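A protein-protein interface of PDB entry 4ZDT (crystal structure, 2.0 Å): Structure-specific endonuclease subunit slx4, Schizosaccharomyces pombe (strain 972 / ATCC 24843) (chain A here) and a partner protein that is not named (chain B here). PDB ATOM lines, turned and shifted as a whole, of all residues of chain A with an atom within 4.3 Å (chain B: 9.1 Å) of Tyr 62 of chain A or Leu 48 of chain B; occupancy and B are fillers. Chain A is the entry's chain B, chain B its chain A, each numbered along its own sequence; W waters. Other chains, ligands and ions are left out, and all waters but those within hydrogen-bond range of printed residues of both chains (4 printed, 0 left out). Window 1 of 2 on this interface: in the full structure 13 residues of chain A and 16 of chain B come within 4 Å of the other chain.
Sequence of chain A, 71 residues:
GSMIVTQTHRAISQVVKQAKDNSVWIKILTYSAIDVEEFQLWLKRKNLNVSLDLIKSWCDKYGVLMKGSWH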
ATOM      1  N   HIS A   9       0.331  10.207  28.510  1.00  0.00           N
ATOM      2  CA  HIS A   9       1.267  10.567  27.450  1.00  0.00           C
ATOM      3  C   HIS A   9       1.943   9.322  26.857  1.00  0.00           C
ATOM      4  O   HIS A   9       2.273   9.288  25.671  1.00  0.00           O
ATOM      5  CB  HIS A   9       2.324  11.540  27.976  1.00  0.00           C
ATOM      6  CG  HIS A   9       1.844  12.954  28.080  1.00  0.00           C
ATOM      7  ND1 HIS A   9       2.575  13.943  28.702  1.00  0.00           N
ATOM      8  CD2 HIS A   9       0.708  13.545  27.642  1.00  0.00           C
ATOM      9  CE1 HIS A   9       1.909  15.083  28.642  1.00  0.00           C
ATOM     10  NE2 HIS A   9       0.772  14.868  28.004  1.00  0.00           N
ATOM     11  N   ILE A  28       6.487  12.084  12.304  1.00  0.00           N
ATOM     12  CA  ILE A  28       7.294  12.496  13.456  1.00  0.00           C
ATOM     13  C   ILE A  28       8.784  12.281  13.167  1.00  0.00           C
ATOM     14  O   ILE A  28       9.604  13.168  13.399  1.00  0.00           O
ATOM     15  CB  ILE A  28       6.885  11.696  14.728  1.00  0.00           C
ATOM     16  CG1 ILE A  28       5.458  12.093  15.163  1.00  0.00           C
ATOM     17  CG2 ILE A  28       7.901  11.890  15.904  1.00  0.00           C
ATOM     18  CD1 ILE A  28       4.837  11.142  16.207  1.00  0.00           C
ATOM     19  N   TYR A  31      10.279  14.899  10.874  1.00  0.00           N
ATOM     20  CA  TYR A  31      10.016  16.282  11.290  1.00  0.00           C
ATOM     21  C   TYR A  31       8.877  16.959  10.499  1.00  0.00           C
ATOM     22  O   TYR A  31       8.936  18.160  10.229  1.00  0.00           O
ATOM     23  CB  TYR A  31      11.319  17.135  11.220  1.00  0.00           C
ATOM     24  CG  TYR A  31      12.486  16.515  11.992  1.00  0.00           C
ATOM     25  CD1 TYR A  31      12.570  16.667  13.375  1.00  0.00           C
ATOM     26  CD2 TYR A  31      13.479  15.790  11.344  1.00  0.00           C
ATOM     27  CE1 TYR A  31      13.613  16.108  14.086  1.00  0.00           C
ATOM     28  CE2 TYR A  31      14.535  15.231  12.046  1.00  0.00           C
ATOM     29  CZ  TYR A  31      14.597  15.383  13.404  1.00  0.00           C
ATOM     30  OH  TYR A  31      15.639  14.820  14.102  1.00  0.00           O
ATOM     31  N   TRP A  58       1.720  16.568  24.927  1.00  0.00           N
ATOM     32  CA  TRP A  58       2.478  15.413  24.464  1.00  0.00           C
ATOM     33  C   TRP A  58       3.428  15.847  23.343  1.00  0.00           C
ATOM     34  O   TRP A  58       4.624  15.587  23.420  1.00  0.00           O
ATOM     35  CB  TRP A  58       1.521  14.296  24.004  1.00  0.00           C
ATOM     36  CG  TRP A  58       2.204  13.069  23.497  1.00  0.00           C
ATOM     37  CD1 TRP A  58       2.721  12.036  24.232  1.00  0.00           C
ATOM     38  CD2 TRP A  58       2.437  12.746  22.126  1.00  0.00           C
ATOM     39  NE1 TRP A  58       3.278  11.092  23.389  1.00  0.00           N
ATOM     40  CE2 TRP A  58       3.108  11.508  22.093  1.00  0.00           C
ATOM     41  CE3 TRP A  58       2.129  13.384  20.915  1.00  0.00           C
ATOM     42  CZ2 TRP A  58       3.491  10.887  20.887  1.00  0.00           C
ATOM     43  CZ3 TRP A  58       2.495  12.764  19.722  1.00  0.00           C
ATOM     44  CH2 TRP A  58       3.168  11.525  19.725  1.00  0.00           C
ATOM     45  N   CYS A  59       2.898  16.535  22.332  1.00  0.00           N
ATOM     46  CA  CYS A  59       3.716  17.006  21.211  1.00  0.00           C
ATOM     47  C   CYS A  59       4.864  17.885  21.701  1.00  0.00           C
ATOM     48  O   CYS A  59       6.020  17.711  21.273  1.00  0.00           O
ATOM     49  CB  CYS A  59       2.895  17.775  20.161  1.00  0.00           C
ATOM     50  SG  CYS A  59       1.682  16.852  19.185  1.00  0.00           S
ATOM     51  N   ASP A  60       4.557  18.822  22.604  1.00  0.00           N
ATOM     52  CA  ASP A  60       5.573  19.753  23.102  1.00  0.00           C
ATOM     53  C   ASP A  60       6.655  19.001  23.841  1.00  0.00           C
ATOM     54  O   ASP A  60       7.828  19.310  23.686  1.00  0.00           O
ATOM     55  CB  ASP A  60       4.965  20.828  24.018  1.00  0.00           C
ATOM     56  CG  ASP A  60       5.911  22.002  24.261  1.00  0.00           C
ATOM     57  OD1 ASP A  60       6.571  22.465  23.297  1.00  0.00           O
ATOM     58  OD2 ASP A  60       5.990  22.463  25.417  1.00  0.00           O
ATOM     59  N   LYS A  61       6.269  18.001  24.632  1.00  0.00           N
ATOM     60  CA  LYS A  61       7.216  17.257  25.452  1.00  0.00           C
ATOM     61  C   LYS A  61       8.088  16.279  24.641  1.00  0.00           C
ATOM     62  O   LYS A  61       9.259  16.074  24.965  1.00  0.00           O
ATOM     63  CB  LYS A  61       6.470  16.521  26.572  1.00  0.00           C
ATOM     64  CG  LYS A  61       7.307  15.612  27.455  1.00  0.00           C
ATOM     65  CD  LYS A  61       8.019  16.393  28.544  1.00  0.00           C
ATOM     66  CE  LYS A  61       8.763  15.477  29.496  1.00  0.00           C
ATOM     67  NZ  LYS A  61       7.844  14.499  30.184  1.00  0.00           N
ATOM     68  N   TYR A  62       7.527  15.695  23.590  1.00  0.00           N
ATOM     69  CA  TYR A  62       8.207  14.602  22.868  1.00  0.00           C
ATOM     70  C   TYR A  62       8.664  14.913  21.433  1.00  0.00           C
ATOM     71  O   TYR A  62       9.117  14.010  20.732  1.00  0.00           O
ATOM     72  CB  TYR A  62       7.351  13.317  22.906  1.00  0.00           C
ATOM     73  CG  TYR A  62       7.156  12.818  24.319  1.00  0.00           C
ATOM     74  CD1 TYR A  62       8.165  12.107  24.977  1.00  0.00           C
ATOM     75  CD2 TYR A  62       5.981  13.091  25.015  1.00  0.00           C
ATOM     76  CE1 TYR A  62       8.005  11.675  26.286  1.00  0.00           C
ATOM     77  CE2 TYR A  62       5.805  12.660  26.328  1.00  0.00           C
ATOM     78  CZ  TYR A  62       6.816  11.959  26.958  1.00  0.00           C
ATOM     79  OH  TYR A  62       6.639  11.535  28.256  1.00  0.00           O
ATOM     80  N   GLY A  63       8.546  16.171  21.007  1.00  0.00           N
ATOM     81  CA  GLY A  63       9.144  16.652  19.761  1.00  0.00           C
ATOM     82  C   GLY A  63       8.306  16.434  18.512  1.00  0.00           C
ATOM     83  O   GLY A  63       8.811  16.040  17.446  1.00  0.00           O
ATOM     84  N   VAL A  64       7.021  16.681  18.627  1.00  0.00           N
ATOM     85  CA  VAL A  64       6.138  16.566  17.476  1.00  0.00           C
ATOM     86  C   VAL A  64       5.671  17.975  17.080  1.00  0.00           C
ATOM     87  O   VAL A  64       5.224  18.742  17.943  1.00  0.00           O
ATOM     88  CB  VAL A  64       4.961  15.637  17.815  1.00  0.00           C
ATOM     89  CG1 VAL A  64       3.976  15.526  16.646  1.00  0.00           C
ATOM     90  CG2 VAL A  64       5.499  14.249  18.244  1.00  0.00           C
ATOM     91  N   LEU B  36      14.945   1.475  12.676  1.00  0.00           N
ATOM     92  CA  LEU B  36      16.080   2.199  13.249  1.00  0.00           C
ATOM     93  C   LEU B  36      15.647   3.025  14.465  1.00  0.00           C
ATOM     94  O   LEU B  36      16.301   3.001  15.496  1.00  0.00           O
ATOM     95  CB  LEU B  36      16.731   3.124  12.195  1.00  0.00           C
ATOM     96  CG  LEU B  36      18.095   3.723  12.564  1.00  0.00           C
ATOM     97  CD1 LEU B  36      19.133   2.633  12.819  1.00  0.00           C
ATOM     98  CD2 LEU B  36      18.605   4.678  11.483  1.00  0.00           C
ATOM     99  N   ALA B  37      14.550   3.765  14.336  1.00  0.00           N
ATOM    100  CA  ALA B  37      14.097   4.595  15.449  1.00  0.00           C
ATOM    101  C   ALA B  37      13.849   3.738  16.692  1.00  0.00           C
ATOM    102  O   ALA B  37      14.337   4.044  17.791  1.00  0.00           O
ATOM    103  CB  ALA B  37      12.845   5.381  15.059  1.00  0.00           C
ATOM    104  N   SER B  38      13.104   2.642  16.507  1.00  0.00           N
ATOM    105  CA  SER B  38      12.829   1.710  17.609  1.00  0.00           C
ATOM    106  C   SER B  38      14.148   1.227  18.288  1.00  0.00           C
ATOM    107  O   SER B  38      14.248   1.191  19.533  1.00  0.00           O
ATOM    108  CB  SER B  38      11.943   0.557  17.106  1.00  0.00           C
ATOM    109  OG  SER B  38      11.646  -0.324  18.156  1.00  0.00           O
ATOM    110  N   PHE B  40      16.895   2.836  18.532  1.00  0.00           N
ATOM    111  CA  PHE B  40      17.555   3.983  19.160  1.00  0.00           C
ATOM    112  C   PHE B  40      16.849   4.449  20.440  1.00  0.00           C
ATOM    113  O   PHE B  40      17.492   5.036  21.317  1.00  0.00           O
ATOM    114  CB  PHE B  40      17.602   5.155  18.186  1.00  0.00           C
ATOM    115  CG  PHE B  40      18.665   5.045  17.110  1.00  0.00           C
ATOM    116  CD1 PHE B  40      19.448   3.905  16.965  1.00  0.00           C
ATOM    117  CD2 PHE B  40      18.865   6.100  16.229  1.00  0.00           C
ATOM    118  CE1 PHE B  40      20.444   3.828  15.965  1.00  0.00           C
ATOM    119  CE2 PHE B  40      19.856   6.034  15.224  1.00  0.00           C
ATOM    120  CZ  PHE B  40      20.637   4.871  15.094  1.00  0.00           C
ATOM    121  N   LEU B  41      15.539   4.196  20.548  1.00  0.00           N
ATOM    122  CA  LEU B  41      14.734   4.698  21.679  1.00  0.00           C
ATOM    123  C   LEU B  41      15.132   4.085  23.032  1.00  0.00           C
ATOM    124  O   LEU B  41      15.377   2.885  23.116  1.00  0.00           O
ATOM    125  CB  LEU B  41      13.219   4.497  21.405  1.00  0.00           C
ATOM    126  CG  LEU B  41      12.644   5.282  20.214  1.00  0.00           C
ATOM    127  CD1 LEU B  41      11.176   4.991  19.983  1.00  0.00           C
ATOM    128  CD2 LEU B  41      12.866   6.783  20.334  1.00  0.00           C
ATOM    129  N   THR B  42      15.186   4.908  24.079  1.00  0.00           N
ATOM    130  CA  THR B  42      15.636   4.451  25.407  1.00  0.00           C
ATOM    131  C   THR B  42      14.504   4.279  26.438  1.00  0.00           C
ATOM    132  O   THR B  42      14.693   3.639  27.477  1.00  0.00           O
ATOM    133  CB  THR B  42      16.783   5.340  25.971  1.00  0.00           C
ATOM    134  OG1 THR B  42      16.411   6.723  25.906  1.00  0.00           O
ATOM    135  CG2 THR B  42      18.064   5.145  25.150  1.00  0.00           C
ATOM    136  N   GLU B  43      13.330   4.832  26.140  1.00  0.00           N
ATOM    137  CA  GLU B  43      12.160   4.715  27.028  1.00  0.00           C
ATOM    138  C   GLU B  43      10.854   4.660  26.227  1.00  0.00           C
ATOM    139  O   GLU B  43      10.770   5.190  25.114  1.00  0.00           O
ATOM    140  CB  GLU B  43      12.144   5.844  28.071  1.00  0.00           C
ATOM    141  CG  GLU B  43      12.392   7.231  27.501  1.00  0.00           C
ATOM    142  CD  GLU B  43      12.380   8.336  28.548  1.00  0.00           C
ATOM    143  OE1 GLU B  43      13.027   8.159  29.609  1.00  0.00           O
ATOM    144  OE2 GLU B  43      11.746   9.396  28.304  1.00  0.00           O
ATOM    145  N   GLU B  44       9.839   4.013  26.796  1.00  0.00           N
ATOM    146  CA  GLU B  44       8.628   3.695  26.041  1.00  0.00           C
ATOM    147  C   GLU B  44       7.763   4.887  25.645  1.00  0.00           C
ATOM    148  O   GLU B  44       7.000   4.801  24.681  1.00  0.00           O
ATOM    149  CB  GLU B  44       7.802   2.615  26.741  1.00  0.00           C
ATOM    150  CG  GLU B  44       8.356   1.182  26.537  1.00  0.00           C
ATOM    151  CD  GLU B  44       8.327   0.674  25.076  1.00  0.00           C
ATOM    152  OE1 GLU B  44       7.807   1.370  24.165  1.00  0.00           O
ATOM    153  OE2 GLU B  44       8.833  -0.452  24.837  1.00  0.00           O
ATOM    154  N   CYS B  45       7.904   6.000  26.360  1.00  0.00           N
ATOM    155  CA  CYS B  45       7.176   7.212  26.018  1.00  0.00           C
ATOM    156  C   CYS B  45       7.778   7.950  24.808  1.00  0.00           C
ATOM    157  O   CYS B  45       7.099   8.741  24.166  1.00  0.00           O
ATOM    158  CB  CYS B  45       7.109   8.128  27.239  1.00  0.00           C
ATOM    159  SG  CYS B  45       8.748   8.440  27.962  1.00  0.00           S
ATOM    160  N   GLN B  46       9.049   7.697  24.498  1.00  0.00           N
ATOM    161  CA  GLN B  46       9.728   8.424  23.415  1.00  0.00           C
ATOM    162  C   GLN B  46       9.293   7.960  22.032  1.00  0.00           C
ATOM    163  O   GLN B  46       9.060   6.763  21.813  1.00  0.00           O
ATOM    164  CB  GLN B  46      11.255   8.300  23.533  1.00  0.00           C
ATOM    165  CG  GLN B  46      11.870   8.967  24.794  1.00  0.00           C
ATOM    166  CD  GLN B  46      11.771  10.510  24.853  1.00  0.00           C
ATOM    167  OE1 GLN B  46      11.836  11.211  23.833  1.00  0.00           O
ATOM    168  NE2 GLN B  46      11.652  11.038  26.074  1.00  0.00           N
ATOM    169  N   VAL B  47       9.206   8.914  21.103  1.00  0.00           N
ATOM    170  CA  VAL B  47       8.862   8.636  19.708  1.00  0.00           C
ATOM    171  C   VAL B  47       9.926   9.138  18.701  1.00  0.00           C
ATOM    172  O   VAL B  47      10.042   8.597  17.592  1.00  0.00           O
ATOM    173  CB  VAL B  47       7.444   9.171  19.320  1.00  0.00           C
ATOM    174  CG1 VAL B  47       6.312   8.292  19.961  1.00  0.00           C
ATOM    175  CG2 VAL B  47       7.252  10.657  19.696  1.00  0.00           C
ATOM    176  N   LEU B  48      10.693  10.150  19.100  1.00  0.00           N
ATOM    177  CA  LEU B  48      11.691  10.779  18.230  1.00  0.00           C
ATOM    178  C   LEU B  48      13.099  10.579  18.794  1.00  0.00           C
ATOM    179  O   LEU B  48      13.439  11.145  19.834  1.00  0.00           O
ATOM    180  CB  LEU B  48      11.400  12.277  18.092  1.00  0.00           C
ATOM    181  CG  LEU B  48      12.344  13.153  17.251  1.00  0.00           C
ATOM    182  CD1 LEU B  48      12.441  12.640  15.826  1.00  0.00           C
ATOM    183  CD2 LEU B  48      11.795  14.565  17.241  1.00  0.00           C
ATOM    184  N   PRO B  49      13.928   9.768  18.115  1.00  0.00           N
ATOM    185  CA  PRO B  49      15.306   9.631  18.582  1.00  0.00           C
ATOM    186  C   PRO B  49      16.065  10.951  18.518  1.00  0.00           C
ATOM    187  O   PRO B  49      15.820  11.765  17.627  1.00  0.00           O
ATOM    188  CB  PRO B  49      15.927   8.638  17.586  1.00  0.00           C
ATOM    189  CG  PRO B  49      14.728   7.899  16.990  1.00  0.00           C
ATOM    190  CD  PRO B  49      13.633   8.911  16.948  1.00  0.00           C
ATOM    191  N   ILE B  50      16.963  11.147  19.476  1.00  0.00           N
ATOM    192  CA  ILE B  50      17.929  12.245  19.452  1.00  0.00           C
ATOM    193  C   ILE B  50      19.199  11.820  18.697  1.00  0.00           C
ATOM    194  O   ILE B  50      19.660  12.505  17.796  1.00  0.00           O
ATOM    195  CB  ILE B  50      18.324  12.662  20.897  1.00  0.00           C
ATOM    196  CG1 ILE B  50      17.081  13.070  21.732  1.00  0.00           C
ATOM    197  CG2 ILE B  50      19.434  13.767  20.893  1.00  0.00           C
ATOM    198  CD1 ILE B  50      16.207  14.138  21.088  1.00  0.00           C
ATOM    199  N   GLU B  51      19.778  10.706  19.118  1.00  0.00           N
ATOM    200  CA  GLU B  51      21.005  10.177  18.512  1.00  0.00           C
ATOM    201  C   GLU B  51      20.999   8.657  18.657  1.00  0.00           C
ATOM    202  O   GLU B  51      20.184   8.100  19.396  1.00  0.00           O
ATOM    203  CB  GLU B  51      22.236  10.755  19.244  1.00  0.00           C
ATOM    204  CG  GLU B  51      22.337  10.315  20.703  1.00  0.00           C
ATOM    205  CD  GLU B  51      23.620  10.784  21.385  1.00  0.00           C
ATOM    206  OE1 GLU B  51      24.531  11.319  20.712  1.00  0.00           O
ATOM    207  OE2 GLU B  51      23.712  10.619  22.614  1.00  0.00           O
ATOM    208  N   ARG B  62      23.465  11.831  15.188  1.00  0.00           N
ATOM    209  CA  ARG B  62      22.142  12.374  15.508  1.00  0.00           C
ATOM    210  C   ARG B  62      21.148  11.820  14.502  1.00  0.00           C
ATOM    211  O   ARG B  62      21.528  11.476  13.371  1.00  0.00           O
ATOM    212  CB  ARG B  62      22.170  13.899  15.420  1.00  0.00           C
ATOM    213  CG  ARG B  62      22.992  14.538  16.531  1.00  0.00           C
ATOM    214  CD  ARG B  62      23.274  16.029  16.306  1.00  0.00           C
ATOM    215  NE  ARG B  62      24.079  16.520  17.436  1.00  0.00           N
ATOM    216  CZ  ARG B  62      24.319  17.812  17.718  1.00  0.00           C
ATOM    217  NH1 ARG B  62      23.834  18.776  16.950  1.00  0.00           N
ATOM    218  NH2 ARG B  62      25.054  18.125  18.779  1.00  0.00           N
ATOM    219  N   TRP B  63      19.880  11.774  14.902  1.00  0.00           N
ATOM    220  CA  TRP B  63      18.815  11.179  14.103  1.00  0.00           C
ATOM    221  C   TRP B  63      18.815  11.713  12.688  1.00  0.00           C
ATOM    222  O   TRP B  63      18.699  10.958  11.721  1.00  0.00           O
ATOM    223  CB  TRP B  63      17.439  11.422  14.767  1.00  0.00           C
ATOM    224  CG  TRP B  63      16.301  10.831  13.968  1.00  0.00           C
ATOM    225  CD1 TRP B  63      15.286  11.507  13.338  1.00  0.00           C
ATOM    226  CD2 TRP B  63      16.112   9.445  13.659  1.00  0.00           C
ATOM    227  NE1 TRP B  63      14.457  10.615  12.675  1.00  0.00           N
ATOM    228  CE2 TRP B  63      14.942   9.345  12.862  1.00  0.00           C
ATOM    229  CE3 TRP B  63      16.811   8.274  13.986  1.00  0.00           C
ATOM    230  CZ2 TRP B  63      14.466   8.118  12.380  1.00  0.00           C
ATOM    231  CZ3 TRP B  63      16.316   7.039  13.513  1.00  0.00           C
ATOM    232  CH2 TRP B  63      15.162   6.982  12.719  1.00  0.00           C
ATOM    233  N   ARG B  64      18.935  13.029  12.560  1.00  0.00           N
ATOM    234  CA  ARG B  64      18.878  13.687  11.257  1.00  0.00           C
ATOM    235  C   ARG B  64      19.874  13.108  10.253  1.00  0.00           C
ATOM    236  O   ARG B  64      19.572  12.990   9.065  1.00  0.00           O
ATOM    237  CB  ARG B  64      19.106  15.192  11.408  1.00  0.00           C
ATOM    238  CG  ARG B  64      18.486  16.028  10.300  1.00  0.00           C
ATOM    239  CD  ARG B  64      18.516  17.509  10.641  1.00  0.00           C
ATOM    240  NE  ARG B  64      17.412  17.897  11.518  1.00  0.00           N
ATOM    241  CZ  ARG B  64      16.173  18.131  11.099  1.00  0.00           C
ATOM    242  NH1 ARG B  64      15.874  18.022   9.812  1.00  0.00           N
ATOM    243  NH2 ARG B  64      15.230  18.474  11.967  1.00  0.00           N
ATOM    244  N   LEU B  67      18.843  10.665   7.655  1.00  0.00           N
ATOM    245  CA  LEU B  67      17.760  11.049   6.754  1.00  0.00           C
ATOM    246  C   LEU B  67      18.216  11.640   5.416  1.00  0.00           C
ATOM    247  O   LEU B  67      17.491  12.457   4.848  1.00  0.00           O
ATOM    248  CB  LEU B  67      16.810  12.049   7.470  1.00  0.00           C
ATOM    249  CG  LEU B  67      16.221  11.647   8.833  1.00  0.00           C
ATOM    250  CD1 LEU B  67      15.344  12.736   9.426  1.00  0.00           C
ATOM    251  CD2 LEU B  67      15.439  10.337   8.734  1.00  0.00           C
HETATM  252  O   HOH W   1      10.148  11.669  21.605  1.00  0.00           O
HETATM  253  O   HOH W   2      11.301  13.784  26.174  1.00  0.00           O
HETATM  254  O   HOH W   3      15.777  14.304  16.680  1.00  0.00           O
HETATM  255  O   HOH W   4      18.894  15.174  14.578  1.00  0.00           O
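The side-chain sulfur (SG) of Cys 45 of chain B lies close to the side-chain hydroxyl (OH) of Tyr 62 of chain A, at 3.8 Å.
The side-chain carboxylate of Glu 43 of chain B is in hydrogen-bond range of the side-chain sulfur of Cys 45 of chain B (3.2 Å). NE2 of Gln 46 of chain B sits at hydrogen-bond distance from OE2 of Glu 43 of chain B (2.8 Å). The backbone carbonyl oxygen of Ile 50 of chain B is in hydrogen-bond range of the backbone NH of Trp 63 of chain B, at 3.0 Å. The backbone carbonyl oxygen (O) of His 9 of chain A is in hydrogen-bond range of the indole nitrogen (NE1) of Trp 58 of chain A (3.1 Å).
Among the printed residues, merely in contact across the chains: Tyr 31 of chain A with Arg 64 of chain B, Gly 63 of chain A with Leu 48 of chain B, Tyr 31 of chain A with Trp 63 of chain B, Tyr 31 of chain A with Leu 67 of chain B, Tyr 62 of chain A with Gln 46 of chain B, Ile 28 of chain A with Leu 48 of chain B, Tyr 62 of chain A with Leu 48 of chain B, Trp 58 of chain A with Val 47 of chain B, Tyr 31 of chain A with Leu 48 of chain B and Tyr 62 of chain A with Val 47 of chain B.
Printed residues of chain B within 4 Å of Tyr 62 of chain A: Cys 45, Gln 46, Val 47 and Leu 48. No residue of chain B comes within 4 Å of Lys 61 of chain A. Gly 63 of chain A touches one residue of chain B. Printed residues of chain B within 4 Å of Tyr 31 of chain A: Leu 48, Trp 63, Arg 64 and Leu 67. Of the printed residues of chain A, Val 47 of chain B touches Trp 58 and Tyr 62. Printed residues of chain B within 4 Å of Ile 28 of chain A: Leu 48 (3.8 Å). Of the printed residues of chain A, Gln 46 of chain B touches Tyr 62. Of the printed residues of chain A, Leu 67 of chain B touches Tyr 31. The nearest printed residue of chain A that does not touch Leu 48 of chain B is Val 64 of chain A (5.4 Å). The nearest printed residue of chain A that does not touch Trp 63 of chain B is Ile 28 of chain A (5.5 Å).
Printed residues of chain A that touch a printed residue of chain B: Ile 28, Tyr 31, Trp 58, Tyr 62 and Gly 63. Hydrophobic or aromatic side chains of chain B that line the printed part of chain A: Val 47, Leu 48, Trp 63 and Leu 67. Among the printed residues, 11 pairs touch across the chains.
Water W3 bridges OH of Tyr 31 of chain A (2.6 Å) and O of Pro 49 of chain B (2.7 Å). Water W1 lies within hydrogen-bond range of O of Tyr 62 of chain A, OE1 of Gln 46 of chain B, N of Val 47 of chain B and N of Leu 48 of chain B. Water W2 lies within hydrogen-bond range of the side-chain amide nitrogen of Gln 46 of chain B and the backbone carbonyl oxygen of Lys 61 of chain A. Water W4 lies within hydrogen-bond range of N of Arg 64 of chain B and OH of Tyr 31 of chain A.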
